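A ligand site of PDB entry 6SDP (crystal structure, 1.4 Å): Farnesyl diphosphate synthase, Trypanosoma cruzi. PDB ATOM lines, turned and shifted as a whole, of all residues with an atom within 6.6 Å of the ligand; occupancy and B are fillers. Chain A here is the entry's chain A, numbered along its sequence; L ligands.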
ATOM      1  N   PHE A  50      12.411  -6.505  18.643  1.00  0.00           N
ATOM      2  CA  PHE A  50      11.948  -6.096  17.323  1.00  0.00           C
ATOM      3  C   PHE A  50      10.451  -5.876  17.317  1.00  0.00           C
ATOM      4  O   PHE A  50       9.948  -4.887  16.751  1.00  0.00           O
ATOM      5  CB  PHE A  50      12.279  -7.161  16.278  1.00  0.00           C
ATOM      6  CG  PHE A  50      13.724  -7.248  15.887  1.00  0.00           C
ATOM      7  CD1 PHE A  50      14.418  -6.118  15.524  1.00  0.00           C
ATOM      8  CD2 PHE A  50      14.369  -8.481  15.836  1.00  0.00           C
ATOM      9  CE1 PHE A  50      15.748  -6.193  15.130  1.00  0.00           C
ATOM     10  CE2 PHE A  50      15.692  -8.577  15.440  1.00  0.00           C
ATOM     11  CZ  PHE A  50      16.375  -7.419  15.106  1.00  0.00           C
ATOM     12  N   ARG A  51       9.702  -6.837  17.853  1.00  0.00           N
ATOM     13  CA  ARG A  51       8.254  -6.814  17.773  1.00  0.00           C
ATOM     14  C   ARG A  51       7.678  -5.692  18.614  1.00  0.00           C
ATOM     15  O   ARG A  51       6.885  -4.881  18.138  1.00  0.00           O
ATOM     16  CB  ARG A  51       7.683  -8.175  18.179  1.00  0.00           C
ATOM     17  CG  ARG A  51       8.112  -9.293  17.246  1.00  0.00           C
ATOM     18  CD  ARG A  51       7.942 -10.643  17.901  1.00  0.00           C
ATOM     19  NE  ARG A  51       8.423 -11.769  17.122  1.00  0.00           N
ATOM     20  CZ  ARG A  51       9.707 -12.098  17.001  1.00  0.00           C
ATOM     21  NH1 ARG A  51      10.073 -13.140  16.259  1.00  0.00           N
ATOM     22  NH2 ARG A  51      10.624 -11.375  17.621  1.00  0.00           N
ATOM     23  N   GLY A  52       8.057  -5.619  19.890  1.00  0.00           N
ATOM     24  CA  GLY A  52       7.493  -4.587  20.743  1.00  0.00           C
ATOM     25  C   GLY A  52       7.864  -3.189  20.274  1.00  0.00           C
ATOM     26  O   GLY A  52       7.047  -2.258  20.306  1.00  0.00           O
ATOM     27  N   THR A  54       8.409  -2.218  17.282  1.00  0.00           N
ATOM     28  CA  THR A  54       7.654  -1.833  16.095  1.00  0.00           C
ATOM     29  C   THR A  54       6.349  -1.127  16.451  1.00  0.00           C
ATOM     30  O   THR A  54       5.941  -0.176  15.761  1.00  0.00           O
ATOM     31  CB  THR A  54       7.438  -3.046  15.198  1.00  0.00           C
ATOM     32  OG1 THR A  54       8.707  -3.478  14.695  1.00  0.00           O
ATOM     33  CG2 THR A  54       6.509  -2.719  14.045  1.00  0.00           C
ATOM     34  N   TYR A 211       2.244 -13.136  14.669  1.00  0.00           N
ATOM     35  CA  TYR A 211       2.678 -12.488  15.912  1.00  0.00           C
ATOM     36  C   TYR A 211       3.920 -11.630  15.723  1.00  0.00           C
ATOM     37  O   TYR A 211       4.143 -10.702  16.516  1.00  0.00           O
ATOM     38  CB  TYR A 211       2.833 -13.499  17.058  1.00  0.00           C
ATOM     39  CG  TYR A 211       4.216 -14.088  17.262  1.00  0.00           C
ATOM     40  CD1 TYR A 211       5.146 -13.470  18.098  1.00  0.00           C
ATOM     41  CD2 TYR A 211       4.615 -15.265  16.618  1.00  0.00           C
ATOM     42  CE1 TYR A 211       6.406 -13.988  18.287  1.00  0.00           C
ATOM     43  CE2 TYR A 211       5.876 -15.803  16.817  1.00  0.00           C
ATOM     44  CZ  TYR A 211       6.770 -15.150  17.647  1.00  0.00           C
ATOM     45  OH  TYR A 211       8.050 -15.665  17.839  1.00  0.00           O
ATOM     46  N   THR A 212       4.733 -11.906  14.706  1.00  0.00           N
ATOM     47  CA  THR A 212       6.013 -11.223  14.524  1.00  0.00           C
ATOM     48  C   THR A 212       5.883  -9.936  13.723  1.00  0.00           C
ATOM     49  O   THR A 212       6.613  -8.978  14.010  1.00  0.00           O
ATOM     50  CB  THR A 212       7.015 -12.199  13.907  1.00  0.00           C
ATOM     51  OG1 THR A 212       7.218 -13.258  14.818  1.00  0.00           O
ATOM     52  CG2 THR A 212       8.341 -11.561  13.642  1.00  0.00           C
ATOM     53  N   TYR A 213       4.958  -9.878  12.762  1.00  0.00           N
ATOM     54  CA  TYR A 213       4.779  -8.690  11.929  1.00  0.00           C
ATOM     55  C   TYR A 213       3.370  -8.151  11.934  1.00  0.00           C
ATOM     56  O   TYR A 213       3.165  -6.935  12.078  1.00  0.00           O
ATOM     57  CB  TYR A 213       5.225  -8.946  10.477  1.00  0.00           C
ATOM     58  CG  TYR A 213       6.722  -9.078  10.363  1.00  0.00           C
ATOM     59  CD1 TYR A 213       7.353 -10.321  10.432  1.00  0.00           C
ATOM     60  CD2 TYR A 213       7.519  -7.956  10.257  1.00  0.00           C
ATOM     61  CE1 TYR A 213       8.734 -10.430  10.364  1.00  0.00           C
ATOM     62  CE2 TYR A 213       8.886  -8.047  10.187  1.00  0.00           C
ATOM     63  CZ  TYR A 213       9.486  -9.285  10.249  1.00  0.00           C
ATOM     64  OH  TYR A 213      10.850  -9.378  10.147  1.00  0.00           O
ATOM     65  N   LEU A 214       2.348  -8.982  11.751  1.00  0.00           N
ATOM     66  CA  LEU A 214       1.005  -8.445  11.647  1.00  0.00           C
ATOM     67  C   LEU A 214       0.593  -7.782  12.957  1.00  0.00           C
ATOM     68  O   LEU A 214       0.125  -6.632  12.973  1.00  0.00           O
ATOM     69  CB  LEU A 214       0.025  -9.549  11.234  1.00  0.00           C
ATOM     70  CG  LEU A 214      -1.398  -9.038  10.990  1.00  0.00           C
ATOM     71  CD1 LEU A 214      -1.534  -8.177   9.775  1.00  0.00           C
ATOM     72  CD2 LEU A 214      -2.348 -10.240  10.910  1.00  0.00           C
ATOM     73  N   PRO A 216       2.399  -6.499  15.621  1.00  0.00           N
ATOM     74  CA  PRO A 216       2.980  -5.190  15.941  1.00  0.00           C
ATOM     75  C   PRO A 216       2.537  -4.089  15.001  1.00  0.00           C
ATOM     76  O   PRO A 216       2.297  -2.981  15.494  1.00  0.00           O
ATOM     77  CB  PRO A 216       4.493  -5.409  15.870  1.00  0.00           C
ATOM     78  CG  PRO A 216       4.711  -6.875  15.818  1.00  0.00           C
ATOM     79  CD  PRO A 216       3.429  -7.541  15.408  1.00  0.00           C
ATOM     80  N   LEU A 217       2.425  -4.342  13.687  1.00  0.00           N
ATOM     81  CA  LEU A 217       2.012  -3.275  12.783  1.00  0.00           C
ATOM     82  C   LEU A 217       0.604  -2.830  13.104  1.00  0.00           C
ATOM     83  O   LEU A 217       0.325  -1.616  13.201  1.00  0.00           O
ATOM     84  CB  LEU A 217       2.108  -3.740  11.337  1.00  0.00           C
ATOM     85  CG  LEU A 217       3.544  -3.922  10.820  1.00  0.00           C
ATOM     86  CD1 LEU A 217       3.529  -4.536   9.431  1.00  0.00           C
ATOM     87  CD2 LEU A 217       4.354  -2.624  10.801  1.00  0.00           C
ATOM     88  N   ILE A 242       7.214 -10.180   4.547  1.00  0.00           N
ATOM     89  CA  ILE A 242       8.398  -9.936   5.362  1.00  0.00           C
ATOM     90  C   ILE A 242       8.587 -11.046   6.381  1.00  0.00           C
ATOM     91  O   ILE A 242       9.720 -11.472   6.657  1.00  0.00           O
ATOM     92  CB  ILE A 242       8.334  -8.542   6.017  1.00  0.00           C
ATOM     93  CG1 ILE A 242       8.220  -7.451   4.952  1.00  0.00           C
ATOM     94  CG2 ILE A 242       9.574  -8.328   6.884  1.00  0.00           C
ATOM     95  CD1 ILE A 242       8.101  -6.058   5.524  1.00  0.00           C
ATOM     96  N   PHE A 246      11.909 -13.391   7.149  1.00  0.00           N
ATOM     97  CA  PHE A 246      12.476 -13.520   8.484  1.00  0.00           C
ATOM     98  C   PHE A 246      12.684 -14.977   8.860  1.00  0.00           C
ATOM     99  O   PHE A 246      13.747 -15.357   9.376  1.00  0.00           O
ATOM    100  CB  PHE A 246      11.526 -12.831   9.476  1.00  0.00           C
ATOM    101  CG  PHE A 246      11.980 -12.834  10.901  1.00  0.00           C
ATOM    102  CD1 PHE A 246      11.596 -13.849  11.759  1.00  0.00           C
ATOM    103  CD2 PHE A 246      12.721 -11.787  11.406  1.00  0.00           C
ATOM    104  CE1 PHE A 246      11.992 -13.823  13.090  1.00  0.00           C
ATOM    105  CE2 PHE A 246      13.118 -11.761  12.736  1.00  0.00           C
ATOM    106  CZ  PHE A 246      12.742 -12.787  13.566  1.00  0.00           C
ATOM    107  N   VAL A 352      10.986   1.024   7.170  1.00  0.00           N
ATOM    108  CA  VAL A 352      11.952   0.864   8.261  1.00  0.00           C
ATOM    109  C   VAL A 352      11.973  -0.570   8.772  1.00  0.00           C
ATOM    110  O   VAL A 352      13.044  -1.138   9.012  1.00  0.00           O
ATOM    111  CB  VAL A 352      11.648   1.865   9.383  1.00  0.00           C
ATOM    112  CG1 VAL A 352      12.495   1.557  10.612  1.00  0.00           C
ATOM    113  CG2 VAL A 352      11.894   3.283   8.898  1.00  0.00           C
ATOM    114  N   VAL A 353      10.800  -1.173   8.967  1.00  0.00           N
ATOM    115  CA  VAL A 353      10.728  -2.574   9.397  1.00  0.00           C
ATOM    116  C   VAL A 353      11.454  -3.471   8.406  1.00  0.00           C
ATOM    117  O   VAL A 353      12.198  -4.384   8.799  1.00  0.00           O
ATOM    118  CB  VAL A 353       9.249  -2.965   9.551  1.00  0.00           C
ATOM    119  CG1 VAL A 353       9.064  -4.455   9.557  1.00  0.00           C
ATOM    120  CG2 VAL A 353       8.681  -2.329  10.787  1.00  0.00           C
ATOM    121  N   TRP A 354      11.244  -3.233   7.107  1.00  0.00           N
ATOM    122  CA  TRP A 354      11.889  -4.073   6.110  1.00  0.00           C
ATOM    123  C   TRP A 354      13.405  -3.904   6.156  1.00  0.00           C
ATOM    124  O   TRP A 354      14.145  -4.898   6.148  1.00  0.00           O
ATOM    125  CB  TRP A 354      11.333  -3.803   4.708  1.00  0.00           C
ATOM    126  CG  TRP A 354      12.214  -4.434   3.650  1.00  0.00           C
ATOM    127  CD1 TRP A 354      12.906  -3.796   2.669  1.00  0.00           C
ATOM    128  CD2 TRP A 354      12.538  -5.823   3.530  1.00  0.00           C
ATOM    129  NE1 TRP A 354      13.632  -4.708   1.933  1.00  0.00           N
ATOM    130  CE2 TRP A 354      13.423  -5.957   2.448  1.00  0.00           C
ATOM    131  CE3 TRP A 354      12.156  -6.963   4.234  1.00  0.00           C
ATOM    132  CZ2 TRP A 354      13.914  -7.193   2.048  1.00  0.00           C
ATOM    133  CZ3 TRP A 354      12.652  -8.179   3.846  1.00  0.00           C
ATOM    134  CH2 TRP A 354      13.532  -8.283   2.763  1.00  0.00           C
ATOM    135  N   GLU A 355      13.885  -2.658   6.219  1.00  0.00           N
ATOM    136  CA  GLU A 355      15.332  -2.470   6.282  1.00  0.00           C
ATOM    137  C   GLU A 355      15.939  -3.172   7.496  1.00  0.00           C
ATOM    138  O   GLU A 355      16.986  -3.814   7.373  1.00  0.00           O
ATOM    139  CB  GLU A 355      15.676  -0.983   6.309  1.00  0.00           C
ATOM    140  CG  GLU A 355      17.164  -0.721   6.217  1.00  0.00           C
ATOM    141  CD  GLU A 355      17.509   0.738   6.356  1.00  0.00           C
ATOM    142  OE1 GLU A 355      18.708   1.083   6.194  1.00  0.00           O
ATOM    143  OE2 GLU A 355      16.592   1.537   6.621  1.00  0.00           O
ATOM    144  N   LYS A 356      15.297  -3.047   8.660  1.00  0.00           N
ATOM    145  CA  LYS A 356      15.791  -3.738   9.860  1.00  0.00           C
ATOM    146  C   LYS A 356      15.834  -5.246   9.639  1.00  0.00           C
ATOM    147  O   LYS A 356      16.823  -5.908   9.953  1.00  0.00           O
ATOM    148  CB  LYS A 356      14.923  -3.395  11.081  1.00  0.00           C
ATOM    149  CG  LYS A 356      15.231  -2.052  11.733  1.00  0.00           C
ATOM    150  CD  LYS A 356      14.300  -1.781  12.919  1.00  0.00           C
ATOM    151  N   THR A 357      14.764  -5.801   9.070  1.00  0.00           N
ATOM    152  CA  THR A 357      14.718  -7.243   8.830  1.00  0.00           C
ATOM    153  C   THR A 357      15.781  -7.671   7.823  1.00  0.00           C
ATOM    154  O   THR A 357      16.480  -8.666   8.011  1.00  0.00           O
ATOM    155  CB  THR A 357      13.323  -7.606   8.317  1.00  0.00           C
ATOM    156  OG1 THR A 357      12.350  -7.246   9.291  1.00  0.00           O
ATOM    157  CG2 THR A 357      13.215  -9.091   8.012  1.00  0.00           C
ATOM    158  N   HIS A 358      15.897  -6.908   6.721  1.00  0.00           N
ATOM    159  CA  HIS A 358      16.834  -7.246   5.658  1.00  0.00           C
ATOM    160  C   HIS A 358      18.266  -7.211   6.155  1.00  0.00           C
ATOM    161  O   HIS A 358      19.107  -8.006   5.711  1.00  0.00           O
ATOM    162  CB  HIS A 358      16.651  -6.228   4.537  1.00  0.00           C
ATOM    163  CG  HIS A 358      17.303  -6.608   3.239  1.00  0.00           C
ATOM    164  ND1 HIS A 358      17.481  -5.701   2.214  1.00  0.00           N
ATOM    165  CD2 HIS A 358      17.802  -7.783   2.801  1.00  0.00           C
ATOM    166  CE1 HIS A 358      18.062  -6.320   1.195  1.00  0.00           C
ATOM    167  NE2 HIS A 358      18.275  -7.574   1.533  1.00  0.00           N
ATOM    168  N   ARG A 360      19.247  -7.654   9.301  1.00  0.00           N
ATOM    169  CA  ARG A 360      19.441  -8.424  10.509  1.00  0.00           C
ATOM    170  C   ARG A 360      20.640  -9.356  10.343  1.00  0.00           C
ATOM    171  O   ARG A 360      20.776 -10.038   9.322  1.00  0.00           O
ATOM    172  CB  ARG A 360      18.182  -9.233  10.787  1.00  0.00           C
ATOM    173  CG  ARG A 360      18.212 -10.018  12.052  1.00  0.00           C
ATOM    174  CD  ARG A 360      16.824 -10.471  12.408  1.00  0.00           C
ATOM    175  NE  ARG A 360      16.275 -11.455  11.485  1.00  0.00           N
ATOM    176  CZ  ARG A 360      16.280 -12.766  11.727  1.00  0.00           C
ATOM    177  NH1 ARG A 360      16.831 -13.247  12.830  1.00  0.00           N
ATOM    178  NH2 ARG A 360      15.712 -13.590  10.863  1.00  0.00           N
HETATM  179  C1  LIG L   1      12.005  -7.221  12.693  1.00  0.00           C
HETATM  180  C2  LIG L   1      11.279  -8.325  13.090  1.00  0.00           C
HETATM  181  C3  LIG L   1       9.971  -8.145  13.491  1.00  0.00           C
HETATM  182  C4  LIG L   1       9.398  -6.881  13.475  1.00  0.00           C
HETATM  183  C5  LIG L   1      10.168  -5.791  13.077  1.00  0.00           C
HETATM  184  C6  LIG L   1      11.480  -5.949  12.688  1.00  0.00           C
HETATM  185  O1  LIG L   1       8.096  -6.671  13.826  1.00  0.00           O
HETATM  186  N1  LIG L   1      13.400  -7.409  12.229  1.00  0.00           N
HETATM  187  O2  LIG L   1      14.062  -6.414  11.981  1.00  0.00           O
HETATM  188  O3  LIG L   1      13.838  -8.545  12.146  1.00  0.00           O
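O1 of the ligand lies within hydrogen-bond range of O of Thr 212, 2.7 Å away.
The backbone NH of Thr 357 is in hydrogen-bond range of an oxygen (O2) of the ligand (3.1 Å).
An oxygen (O2) of the ligand lies within hydrogen-bond range of the side-chain hydroxyl (OG1) of Thr 357 (3.3 Å).
An oxygen (O1) of the ligand lies close to the side-chain hydroxyl (OG1) of Thr 54.
The side-chain hydroxyl of Thr 212 is in hydrogen-bond range of the guanidinium group of Arg 51, 3.0 Å away.
OG1 of Thr 357 is in hydrogen-bond range of OH of Tyr 213, 2.7 Å away.
OG1 of Thr 357 sits at hydrogen-bond distance from O of Val 353 (2.9 Å).
The side-chain hydroxyl (OG1) of Thr 54 is in hydrogen-bond range of the backbone carbonyl oxygen (O) of Phe 50, at 2.8 Å.
The backbone carbonyl oxygen (O) of Phe 246 sits at hydrogen-bond distance from the guanidinium group (NH2) of Arg 360, at 3.0 Å.
O of Lys 356 lies close to O2 of the ligand (3.5 Å).
CB of Phe 50 touches C2 of the ligand, 3.5 Å away.
CA of Arg 51 touches O1 of the ligand, at 3.95 Å.
Tyr 213 touches the ligand (OH to C2, 3.2 Å).
Pro 216 touches the ligand (CG to O1, 3.9 Å).
Phe 246 touches the ligand.
CG1 of Val 353 touches C5 of the ligand, 3.9 Å away.
Arg 360 touches the ligand (CD to O3, 3.6 Å).
Hydrophobic or aromatic side chains that line the ligand: Phe 50, Tyr 213, Pro 216, Phe 246 and Val 353.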
